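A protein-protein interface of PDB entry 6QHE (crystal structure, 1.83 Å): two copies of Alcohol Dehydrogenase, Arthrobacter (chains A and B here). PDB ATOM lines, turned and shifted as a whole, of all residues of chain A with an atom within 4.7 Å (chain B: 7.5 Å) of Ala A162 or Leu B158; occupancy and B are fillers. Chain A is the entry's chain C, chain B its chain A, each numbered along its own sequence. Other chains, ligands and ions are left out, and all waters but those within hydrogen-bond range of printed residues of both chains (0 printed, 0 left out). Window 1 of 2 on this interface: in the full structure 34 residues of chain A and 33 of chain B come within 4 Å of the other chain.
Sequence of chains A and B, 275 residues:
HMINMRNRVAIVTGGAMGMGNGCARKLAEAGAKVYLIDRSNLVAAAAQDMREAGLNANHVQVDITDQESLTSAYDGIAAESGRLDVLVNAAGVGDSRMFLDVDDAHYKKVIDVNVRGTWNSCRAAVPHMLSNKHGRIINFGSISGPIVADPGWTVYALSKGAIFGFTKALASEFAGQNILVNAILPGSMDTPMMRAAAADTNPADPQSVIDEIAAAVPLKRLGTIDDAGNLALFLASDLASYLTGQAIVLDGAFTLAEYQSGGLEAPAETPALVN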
ATOM      1  N   VAL A 115     -21.615 -26.474 -31.885  1.00  0.00           N
ATOM      2  CA  VAL A 115     -20.191 -26.090 -32.058  1.00  0.00           C
ATOM      3  C   VAL A 115     -19.772 -26.347 -33.507  1.00  0.00           C
ATOM      4  O   VAL A 115     -19.446 -25.378 -34.214  1.00  0.00           O
ATOM      5  CB  VAL A 115     -19.281 -26.814 -31.050  1.00  0.00           C
ATOM      6  CG1 VAL A 115     -17.842 -26.348 -31.201  1.00  0.00           C
ATOM      7  CG2 VAL A 115     -19.759 -26.577 -29.622  1.00  0.00           C
ATOM      8  N   TRP A 119     -18.954 -23.751 -36.501  1.00  0.00           N
ATOM      9  CA  TRP A 119     -17.603 -23.849 -37.119  1.00  0.00           C
ATOM     10  C   TRP A 119     -17.752 -23.961 -38.643  1.00  0.00           C
ATOM     11  O   TRP A 119     -17.169 -23.140 -39.384  1.00  0.00           O
ATOM     12  CB  TRP A 119     -16.831 -25.033 -36.551  1.00  0.00           C
ATOM     13  CG  TRP A 119     -15.501 -25.164 -37.217  1.00  0.00           C
ATOM     14  CD1 TRP A 119     -15.239 -25.776 -38.402  1.00  0.00           C
ATOM     15  CD2 TRP A 119     -14.259 -24.629 -36.738  1.00  0.00           C
ATOM     16  NE1 TRP A 119     -13.914 -25.626 -38.718  1.00  0.00           N
ATOM     17  CE2 TRP A 119     -13.282 -24.964 -37.700  1.00  0.00           C
ATOM     18  CE3 TRP A 119     -13.875 -23.971 -35.566  1.00  0.00           C
ATOM     19  CZ2 TRP A 119     -11.951 -24.604 -37.545  1.00  0.00           C
ATOM     20  CZ3 TRP A 119     -12.549 -23.635 -35.398  1.00  0.00           C
ATOM     21  CH2 TRP A 119     -11.614 -23.917 -36.392  1.00  0.00           C
ATOM     22  N   LEU A 158     -21.305 -26.373 -22.002  1.00  0.00           N
ATOM     23  CA  LEU A 158     -20.000 -26.630 -22.669  1.00  0.00           C
ATOM     24  C   LEU A 158     -20.063 -26.086 -24.104  1.00  0.00           C
ATOM     25  O   LEU A 158     -19.147 -25.328 -24.503  1.00  0.00           O
ATOM     26  CB  LEU A 158     -19.752 -28.144 -22.605  1.00  0.00           C
ATOM     27  CG  LEU A 158     -18.444 -28.667 -23.191  1.00  0.00           C
ATOM     28  CD1 LEU A 158     -18.188 -30.076 -22.693  1.00  0.00           C
ATOM     29  CD2 LEU A 158     -18.463 -28.630 -24.708  1.00  0.00           C
ATOM     30  N   SER A 159     -21.140 -26.377 -24.852  1.00  0.00           N
ATOM     31  CA  SER A 159     -21.270 -25.964 -26.261  1.00  0.00           C
ATOM     32  C   SER A 159     -21.302 -24.431 -26.344  1.00  0.00           C
ATOM     33  O   SER A 159     -20.671 -23.847 -27.282  1.00  0.00           O
ATOM     34  CB  SER A 159     -22.465 -26.610 -26.952  1.00  0.00           C
ATOM     35  OG  SER A 159     -23.707 -25.992 -26.620  1.00  0.00           O
ATOM     36  N   LYS A 160     -21.961 -23.757 -25.410  1.00  0.00           N
ATOM     37  CA  LYS A 160     -22.129 -22.281 -25.498  1.00  0.00           C
ATOM     38  C   LYS A 160     -20.875 -21.591 -24.972  1.00  0.00           C
ATOM     39  O   LYS A 160     -20.546 -20.491 -25.461  1.00  0.00           O
ATOM     40  CB  LYS A 160     -23.435 -21.894 -24.807  1.00  0.00           C
ATOM     41  CG  LYS A 160     -24.701 -22.447 -25.493  1.00  0.00           C
ATOM     42  CD  LYS A 160     -24.729 -22.171 -26.969  1.00  0.00           C
ATOM     43  CE  LYS A 160     -26.080 -22.396 -27.627  1.00  0.00           C
ATOM     44  NZ  LYS A 160     -26.099 -21.878 -29.016  1.00  0.00           N
ATOM     45  N   GLY A 161     -20.154 -22.214 -24.048  1.00  0.00           N
ATOM     46  CA  GLY A 161     -18.817 -21.728 -23.674  1.00  0.00           C
ATOM     47  C   GLY A 161     -17.883 -21.829 -24.879  1.00  0.00           C
ATOM     48  O   GLY A 161     -17.065 -20.898 -25.112  1.00  0.00           O
ATOM     49  N   ALA A 162     -17.965 -22.914 -25.630  1.00  0.00           N
ATOM     50  CA  ALA A 162     -17.152 -23.084 -26.863  1.00  0.00           C
ATOM     51  C   ALA A 162     -17.450 -21.942 -27.834  1.00  0.00           C
ATOM     52  O   ALA A 162     -16.502 -21.358 -28.386  1.00  0.00           O
ATOM     53  CB  ALA A 162     -17.416 -24.438 -27.471  1.00  0.00           C
ATOM     54  N   ILE A 163     -18.728 -21.614 -28.051  1.00  0.00           N
ATOM     55  CA  ILE A 163     -19.117 -20.491 -28.947  1.00  0.00           C
ATOM     56  C   ILE A 163     -18.533 -19.172 -28.423  1.00  0.00           C
ATOM     57  O   ILE A 163     -18.053 -18.378 -29.239  1.00  0.00           O
ATOM     58  CB  ILE A 163     -20.657 -20.413 -29.106  1.00  0.00           C
ATOM     59  CG1 ILE A 163     -21.198 -21.624 -29.867  1.00  0.00           C
ATOM     60  CG2 ILE A 163     -21.072 -19.129 -29.777  1.00  0.00           C
ATOM     61  CD1 ILE A 163     -20.464 -21.891 -31.164  1.00  0.00           C
ATOM     62  N   PHE A 164     -18.576 -18.951 -27.121  1.00  0.00           N
ATOM     63  CA  PHE A 164     -18.043 -17.723 -26.478  1.00  0.00           C
ATOM     64  C   PHE A 164     -16.557 -17.581 -26.851  1.00  0.00           C
ATOM     65  O   PHE A 164     -16.130 -16.528 -27.365  1.00  0.00           O
ATOM     66  CB  PHE A 164     -18.272 -17.807 -24.970  1.00  0.00           C
ATOM     67  CG  PHE A 164     -17.919 -16.559 -24.202  1.00  0.00           C
ATOM     68  CD1 PHE A 164     -18.892 -15.609 -23.922  1.00  0.00           C
ATOM     69  CD2 PHE A 164     -16.668 -16.379 -23.651  1.00  0.00           C
ATOM     70  CE1 PHE A 164     -18.607 -14.478 -23.172  1.00  0.00           C
ATOM     71  CE2 PHE A 164     -16.377 -15.251 -22.899  1.00  0.00           C
ATOM     72  CZ  PHE A 164     -17.349 -14.301 -22.649  1.00  0.00           C
ATOM     73  N   GLY A 165     -15.774 -18.622 -26.617  1.00  0.00           N
ATOM     74  CA  GLY A 165     -14.321 -18.613 -26.879  1.00  0.00           C
ATOM     75  C   GLY A 165     -14.020 -18.518 -28.348  1.00  0.00           C
ATOM     76  O   GLY A 165     -13.111 -17.736 -28.745  1.00  0.00           O
ATOM     77  N   PHE A 166     -14.721 -19.312 -29.162  1.00  0.00           N
ATOM     78  CA  PHE A 166     -14.533 -19.308 -30.631  1.00  0.00           C
ATOM     79  C   PHE A 166     -14.826 -17.919 -31.197  1.00  0.00           C
ATOM     80  O   PHE A 166     -14.058 -17.427 -32.052  1.00  0.00           O
ATOM     81  CB  PHE A 166     -15.405 -20.377 -31.277  1.00  0.00           C
ATOM     82  CG  PHE A 166     -15.384 -20.338 -32.773  1.00  0.00           C
ATOM     83  CD1 PHE A 166     -14.206 -20.600 -33.446  1.00  0.00           C
ATOM     84  CD2 PHE A 166     -16.517 -20.045 -33.502  1.00  0.00           C
ATOM     85  CE1 PHE A 166     -14.159 -20.548 -34.836  1.00  0.00           C
ATOM     86  CE2 PHE A 166     -16.500 -20.052 -34.891  1.00  0.00           C
ATOM     87  CZ  PHE A 166     -15.293 -20.254 -35.556  1.00  0.00           C
ATOM     88  N   TYR B 107      -8.329 -30.052 -35.494  1.00  0.00           N
ATOM     89  CA  TYR B 107      -9.598 -29.767 -34.774  1.00  0.00           C
ATOM     90  C   TYR B 107      -9.831 -30.888 -33.757  1.00  0.00           C
ATOM     91  O   TYR B 107     -10.058 -30.626 -32.571  1.00  0.00           O
ATOM     92  CB  TYR B 107     -10.745 -29.661 -35.772  1.00  0.00           C
ATOM     93  CG  TYR B 107     -12.090 -29.340 -35.178  1.00  0.00           C
ATOM     94  CD1 TYR B 107     -12.919 -30.311 -34.651  1.00  0.00           C
ATOM     95  CD2 TYR B 107     -12.516 -28.019 -35.134  1.00  0.00           C
ATOM     96  CE1 TYR B 107     -14.176 -29.989 -34.144  1.00  0.00           C
ATOM     97  CE2 TYR B 107     -13.756 -27.678 -34.607  1.00  0.00           C
ATOM     98  CZ  TYR B 107     -14.576 -28.660 -34.091  1.00  0.00           C
ATOM     99  OH  TYR B 107     -15.788 -28.292 -33.584  1.00  0.00           O
ATOM    100  N   VAL B 110      -6.977 -31.219 -30.687  1.00  0.00           N
ATOM    101  CA  VAL B 110      -7.073 -30.182 -29.627  1.00  0.00           C
ATOM    102  C   VAL B 110      -8.357 -30.399 -28.824  1.00  0.00           C
ATOM    103  O   VAL B 110      -8.269 -30.402 -27.577  1.00  0.00           O
ATOM    104  CB  VAL B 110      -6.982 -28.776 -30.215  1.00  0.00           C
ATOM    105  CG1 VAL B 110      -7.164 -27.719 -29.145  1.00  0.00           C
ATOM    106  CG2 VAL B 110      -5.677 -28.545 -30.979  1.00  0.00           C
ATOM    107  N   ILE B 111      -9.490 -30.592 -29.490  1.00  0.00           N
ATOM    108  CA  ILE B 111     -10.787 -30.698 -28.759  1.00  0.00           C
ATOM    109  C   ILE B 111     -10.888 -32.029 -28.019  1.00  0.00           C
ATOM    110  O   ILE B 111     -11.362 -32.025 -26.873  1.00  0.00           O
ATOM    111  CB  ILE B 111     -11.957 -30.402 -29.703  1.00  0.00           C
ATOM    112  CG1 ILE B 111     -11.880 -28.933 -30.119  1.00  0.00           C
ATOM    113  CG2 ILE B 111     -13.290 -30.787 -29.082  1.00  0.00           C
ATOM    114  CD1 ILE B 111     -12.699 -28.582 -31.316  1.00  0.00           C
ATOM    115  N   ASN B 114      -8.402 -31.522 -24.847  1.00  0.00           N
ATOM    116  CA  ASN B 114      -8.723 -30.358 -23.976  1.00  0.00           C
ATOM    117  C   ASN B 114     -10.148 -30.488 -23.432  1.00  0.00           C
ATOM    118  O   ASN B 114     -10.358 -30.143 -22.264  1.00  0.00           O
ATOM    119  CB  ASN B 114      -8.487 -29.033 -24.688  1.00  0.00           C
ATOM    120  CG  ASN B 114      -7.012 -28.763 -24.927  1.00  0.00           C
ATOM    121  OD1 ASN B 114      -6.160 -29.586 -24.554  1.00  0.00           O
ATOM    122  ND2 ASN B 114      -6.700 -27.616 -25.529  1.00  0.00           N
ATOM    123  N   VAL B 115     -11.091 -30.912 -24.259  1.00  0.00           N
ATOM    124  CA  VAL B 115     -12.528 -30.954 -23.894  1.00  0.00           C
ATOM    125  C   VAL B 115     -12.908 -32.370 -23.473  1.00  0.00           C
ATOM    126  O   VAL B 115     -13.245 -32.570 -22.282  1.00  0.00           O
ATOM    127  CB  VAL B 115     -13.433 -30.416 -25.010  1.00  0.00           C
ATOM    128  CG1 VAL B 115     -14.895 -30.385 -24.557  1.00  0.00           C
ATOM    129  CG2 VAL B 115     -12.987 -29.021 -25.420  1.00  0.00           C
ATOM    130  N   SER B 144      -6.959 -17.431 -23.052  1.00  0.00           N
ATOM    131  CA  SER B 144      -7.250 -17.513 -24.503  1.00  0.00           C
ATOM    132  C   SER B 144      -8.623 -18.147 -24.733  1.00  0.00           C
ATOM    133  O   SER B 144      -8.755 -19.379 -24.471  1.00  0.00           O
ATOM    134  CB  SER B 144      -6.180 -18.261 -25.256  1.00  0.00           C
ATOM    135  OG  SER B 144      -6.539 -18.388 -26.633  1.00  0.00           O
ATOM    136  N   GLY B 145      -9.579 -17.341 -25.201  1.00  0.00           N
ATOM    137  CA  GLY B 145     -10.973 -17.758 -25.431  1.00  0.00           C
ATOM    138  C   GLY B 145     -11.931 -16.987 -24.537  1.00  0.00           C
ATOM    139  O   GLY B 145     -12.657 -16.138 -25.022  1.00  0.00           O
ATOM    140  N   PRO B 146     -11.910 -17.226 -23.217  1.00  0.00           N
ATOM    141  CA  PRO B 146     -12.792 -16.519 -22.303  1.00  0.00           C
ATOM    142  C   PRO B 146     -12.449 -15.037 -22.108  1.00  0.00           C
ATOM    143  O   PRO B 146     -13.362 -14.257 -21.862  1.00  0.00           O
ATOM    144  CB  PRO B 146     -12.637 -17.241 -20.973  1.00  0.00           C
ATOM    145  CG  PRO B 146     -11.924 -18.517 -21.265  1.00  0.00           C
ATOM    146  CD  PRO B 146     -11.172 -18.311 -22.563  1.00  0.00           C
ATOM    147  N   TRP B 153      -5.553 -19.058 -33.058  1.00  0.00           N
ATOM    148  CA  TRP B 153      -5.870 -19.858 -31.854  1.00  0.00           C
ATOM    149  C   TRP B 153      -7.351 -20.242 -31.824  1.00  0.00           C
ATOM    150  O   TRP B 153      -7.811 -20.535 -30.721  1.00  0.00           O
ATOM    151  CB  TRP B 153      -5.490 -19.073 -30.608  1.00  0.00           C
ATOM    152  CG  TRP B 153      -4.018 -18.848 -30.484  1.00  0.00           C
ATOM    153  CD1 TRP B 153      -3.322 -17.743 -30.884  1.00  0.00           C
ATOM    154  CD2 TRP B 153      -3.038 -19.784 -30.005  1.00  0.00           C
ATOM    155  NE1 TRP B 153      -1.980 -17.913 -30.646  1.00  0.00           N
ATOM    156  CE2 TRP B 153      -1.773 -19.157 -30.123  1.00  0.00           C
ATOM    157  CE3 TRP B 153      -3.089 -21.096 -29.527  1.00  0.00           C
ATOM    158  CZ2 TRP B 153      -0.588 -19.786 -29.743  1.00  0.00           C
ATOM    159  CZ3 TRP B 153      -1.923 -21.712 -29.122  1.00  0.00           C
ATOM    160  CH2 TRP B 153      -0.685 -21.063 -29.237  1.00  0.00           C
ATOM    161  N   THR B 154      -8.059 -20.277 -32.957  1.00  0.00           N
ATOM    162  CA  THR B 154      -9.527 -20.529 -32.942  1.00  0.00           C
ATOM    163  C   THR B 154      -9.841 -21.864 -32.247  1.00  0.00           C
ATOM    164  O   THR B 154     -10.789 -21.898 -31.437  1.00  0.00           O
ATOM    165  CB  THR B 154     -10.153 -20.455 -34.336  1.00  0.00           C
ATOM    166  OG1 THR B 154      -9.469 -21.320 -35.260  1.00  0.00           O
ATOM    167  CG2 THR B 154     -10.220 -19.041 -34.857  1.00  0.00           C
ATOM    168  N   VAL B 155      -9.146 -22.968 -32.560  1.00  0.00           N
ATOM    169  CA  VAL B 155      -9.533 -24.272 -31.980  1.00  0.00           C
ATOM    170  C   VAL B 155      -9.177 -24.303 -30.494  1.00  0.00           C
ATOM    171  O   VAL B 155      -9.973 -24.770 -29.683  1.00  0.00           O
ATOM    172  CB  VAL B 155      -8.916 -25.463 -32.741  1.00  0.00           C
ATOM    173  CG1 VAL B 155      -9.311 -26.771 -32.094  1.00  0.00           C
ATOM    174  CG2 VAL B 155      -9.351 -25.438 -34.201  1.00  0.00           C
ATOM    175  N   TYR B 156      -7.993 -23.837 -30.126  1.00  0.00           N
ATOM    176  CA  TYR B 156      -7.584 -23.814 -28.704  1.00  0.00           C
ATOM    177  C   TYR B 156      -8.575 -22.950 -27.914  1.00  0.00           C
ATOM    178  O   TYR B 156      -9.043 -23.398 -26.837  1.00  0.00           O
ATOM    179  CB  TYR B 156      -6.166 -23.280 -28.583  1.00  0.00           C
ATOM    180  CG  TYR B 156      -5.627 -23.288 -27.185  1.00  0.00           C
ATOM    181  CD1 TYR B 156      -5.114 -24.435 -26.612  1.00  0.00           C
ATOM    182  CD2 TYR B 156      -5.565 -22.123 -26.444  1.00  0.00           C
ATOM    183  CE1 TYR B 156      -4.593 -24.438 -25.334  1.00  0.00           C
ATOM    184  CE2 TYR B 156      -5.007 -22.097 -25.175  1.00  0.00           C
ATOM    185  CZ  TYR B 156      -4.524 -23.249 -24.613  1.00  0.00           C
ATOM    186  OH  TYR B 156      -4.040 -23.244 -23.337  1.00  0.00           O
ATOM    187  N   ALA B 157      -8.872 -21.758 -28.412  1.00  0.00           N
ATOM    188  CA  ALA B 157      -9.765 -20.796 -27.714  1.00  0.00           C
ATOM    189  C   ALA B 157     -11.180 -21.402 -27.577  1.00  0.00           C
ATOM    190  O   ALA B 157     -11.800 -21.289 -26.503  1.00  0.00           O
ATOM    191  CB  ALA B 157      -9.785 -19.487 -28.432  1.00  0.00           C
ATOM    192  N   LEU B 158     -11.670 -22.053 -28.627  1.00  0.00           N
ATOM    193  CA  LEU B 158     -12.953 -22.818 -28.578  1.00  0.00           C
ATOM    194  C   LEU B 158     -12.863 -23.860 -27.461  1.00  0.00           C
ATOM    195  O   LEU B 158     -13.804 -23.924 -26.622  1.00  0.00           O
ATOM    196  CB  LEU B 158     -13.153 -23.414 -29.973  1.00  0.00           C
ATOM    197  CG  LEU B 158     -14.389 -24.264 -30.227  1.00  0.00           C
ATOM    198  CD1 LEU B 158     -14.560 -24.452 -31.739  1.00  0.00           C
ATOM    199  CD2 LEU B 158     -14.314 -25.612 -29.532  1.00  0.00           C
ATOM    200  N   SER B 159     -11.771 -24.625 -27.378  1.00  0.00           N
ATOM    201  CA  SER B 159     -11.613 -25.700 -26.373  1.00  0.00           C
ATOM    202  C   SER B 159     -11.630 -25.102 -24.954  1.00  0.00           C
ATOM    203  O   SER B 159     -12.253 -25.689 -24.028  1.00  0.00           O
ATOM    204  CB  SER B 159     -10.372 -26.559 -26.661  1.00  0.00           C
ATOM    205  OG  SER B 159      -9.177 -25.951 -26.202  1.00  0.00           O
ATOM    206  N   LYS B 160     -11.015 -23.945 -24.762  1.00  0.00           N
ATOM    207  CA  LYS B 160     -10.883 -23.362 -23.390  1.00  0.00           C
ATOM    208  C   LYS B 160     -12.179 -22.610 -23.033  1.00  0.00           C
ATOM    209  O   LYS B 160     -12.520 -22.567 -21.851  1.00  0.00           O
ATOM    210  CB  LYS B 160      -9.607 -22.523 -23.322  1.00  0.00           C
ATOM    211  CG  LYS B 160      -8.325 -23.333 -23.511  1.00  0.00           C
ATOM    212  CD  LYS B 160      -8.267 -24.538 -22.602  1.00  0.00           C
ATOM    213  CE  LYS B 160      -6.893 -25.171 -22.471  1.00  0.00           C
ATOM    214  NZ  LYS B 160      -6.870 -26.177 -21.383  1.00  0.00           N
ATOM    215  N   GLY B 161     -12.895 -22.101 -24.016  1.00  0.00           N
ATOM    216  CA  GLY B 161     -14.261 -21.590 -23.795  1.00  0.00           C
ATOM    217  C   GLY B 161     -15.175 -22.722 -23.348  1.00  0.00           C
ATOM    218  O   GLY B 161     -15.991 -22.534 -22.419  1.00  0.00           O
ATOM    219  N   ALA B 162     -15.040 -23.893 -23.976  1.00  0.00           N
ATOM    220  CA  ALA B 162     -15.813 -25.087 -23.594  1.00  0.00           C
ATOM    221  C   ALA B 162     -15.544 -25.417 -22.121  1.00  0.00           C
ATOM    222  O   ALA B 162     -16.495 -25.696 -21.367  1.00  0.00           O
ATOM    223  CB  ALA B 162     -15.460 -26.217 -24.512  1.00  0.00           C
ATOM    224  N   ILE B 163     -14.271 -25.414 -21.701  1.00  0.00           N
ATOM    225  CA  ILE B 163     -13.905 -25.721 -20.300  1.00  0.00           C
ATOM    226  C   ILE B 163     -14.539 -24.674 -19.363  1.00  0.00           C
ATOM    227  O   ILE B 163     -15.041 -25.048 -18.304  1.00  0.00           O
ATOM    228  CB  ILE B 163     -12.373 -25.785 -20.131  1.00  0.00           C
ATOM    229  CG1 ILE B 163     -11.771 -26.988 -20.851  1.00  0.00           C
ATOM    230  CG2 ILE B 163     -11.997 -25.813 -18.658  1.00  0.00           C
ATOM    231  CD1 ILE B 163     -12.423 -28.247 -20.561  1.00  0.00           C
ATOM    232  N   PHE B 164     -14.513 -23.406 -19.746  1.00  0.00           N
ATOM    233  CA  PHE B 164     -15.101 -22.301 -18.953  1.00  0.00           C
ATOM    234  C   PHE B 164     -16.586 -22.613 -18.681  1.00  0.00           C
ATOM    235  O   PHE B 164     -17.033 -22.627 -17.515  1.00  0.00           O
ATOM    236  CB  PHE B 164     -14.894 -20.994 -19.718  1.00  0.00           C
ATOM    237  CG  PHE B 164     -15.320 -19.743 -19.004  1.00  0.00           C
ATOM    238  CD1 PHE B 164     -14.422 -19.042 -18.207  1.00  0.00           C
ATOM    239  CD2 PHE B 164     -16.598 -19.224 -19.143  1.00  0.00           C
ATOM    240  CE1 PHE B 164     -14.791 -17.854 -17.593  1.00  0.00           C
ATOM    241  CE2 PHE B 164     -16.983 -18.072 -18.460  1.00  0.00           C
ATOM    242  CZ  PHE B 164     -16.078 -17.373 -17.701  1.00  0.00           C
ATOM    243  N   GLY B 165     -17.351 -22.902 -19.739  1.00  0.00           N
ATOM    244  CA  GLY B 165     -18.798 -23.155 -19.624  1.00  0.00           C
ATOM    245  C   GLY B 165     -19.078 -24.448 -18.890  1.00  0.00           C
ATOM    246  O   GLY B 165     -20.009 -24.485 -18.055  1.00  0.00           O
ATOM    247  N   PHE B 166     -18.317 -25.493 -19.188  1.00  0.00           N
ATOM    248  CA  PHE B 166     -18.477 -26.826 -18.559  1.00  0.00           C
ATOM    249  C   PHE B 166     -18.239 -26.701 -17.068  1.00  0.00           C
ATOM    250  O   PHE B 166     -18.994 -27.271 -16.256  1.00  0.00           O
ATOM    251  CB  PHE B 166     -17.543 -27.845 -19.211  1.00  0.00           C
ATOM    252  CG  PHE B 166     -17.517 -29.166 -18.503  1.00  0.00           C
ATOM    253  CD1 PHE B 166     -18.672 -29.926 -18.408  1.00  0.00           C
ATOM    254  CD2 PHE B 166     -16.365 -29.624 -17.901  1.00  0.00           C
ATOM    255  CE1 PHE B 166     -18.664 -31.134 -17.735  1.00  0.00           C
ATOM    256  CE2 PHE B 166     -16.352 -30.849 -17.244  1.00  0.00           C
ATOM    257  CZ  PHE B 166     -17.520 -31.586 -17.150  1.00  0.00           C
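O of Gly B161 sits close to O of Gly A161, 3.3 Å away.
N of Ala A162 sits close to N of Ala B162 (3.5 Å).
Among the printed residues, merely in contact across the chains: Val A115 with Tyr B107, Val A115 with Leu B158, Trp A119 with Tyr B107, Trp A119 with Thr B154, Trp A119 with Val B155, Trp A119 with Leu B158, Leu A158 with Val B115, Leu A158 with Ala B162, Gly A161 with Ala B162, Ala A162 with Leu B158, Ala A162 with Gly B161, Phe A164 with Pro B146, Gly A165 with Gly B145, Gly A165 with Ala B157 and Phe A166 with Leu B158.
Of the printed residues of chain B, Leu A158 touches Val B115 and Ala B162.
Of chain B, only Gly B161 (3.2 Å) and Ala B162 (3.6 Å) come within 4 Å of Gly A161.
Of chain B, only Leu B158, Gly B161 and Ala B162 come within 4 Å of Ala A162.
Printed residues of chain A within 4 Å of Tyr B107: Val A115 and Trp A119.
Asn B114 touches none of the printed residues of chain A.
Of chain A, only Val A115, Trp A119, Ala A162 and Phe A166 come within 4 Å of Leu B158.
Of the printed residues of chain A, Ala B162 touches Leu A158, Gly A161 and Ala A162.
Phe B164 touches none of the printed residues of chain A.
The nearest residue of chain B that does not touch Ala A162 is Ala B157 (5.1 Å).
The nearest residue of chain A that does not touch Leu B158 is Gly A165 (4.3 Å).
The nearest printed residue of chain A that does not touch Pro B146 is Gly A165 (4.6 Å).
Printed residues of chain B that touch a printed residue of chain A: Tyr B107, Val B115, Gly B145, Pro B146, Thr B154, Val B155, Ala B157, Leu B158, Gly B161 and Ala B162.
Printed residues of chain A that touch a printed residue of chain B: Val A115, Trp A119, Leu A158, Gly A161, Ala A162, Phe A164, Gly A165 and Phe A166.
Hydrophobic or aromatic side chains of chain A that line the printed part of chain B: Val A115, Trp A119, Leu A158, Ala A162, Phe A164 and Phe A166.
Among the printed residues, 17 pairs touch across the chains.
Val A115 touches Leu B158, and with the chains exchanged Leu A158 touches Val B115.
Gly B161 touches its own counterpart, Gly A161.
Gly A161 touches Ala B162, and with the chains exchanged Ala A162 touches Gly B161.
Phe A166 touches Leu B158, but with the chains exchanged Leu A158 does not touch Phe B166 (4.03 Å).
Of the 17 pairs that touch across the chains among the printed residues, 8 have their exchanged pair printed and touching as well.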
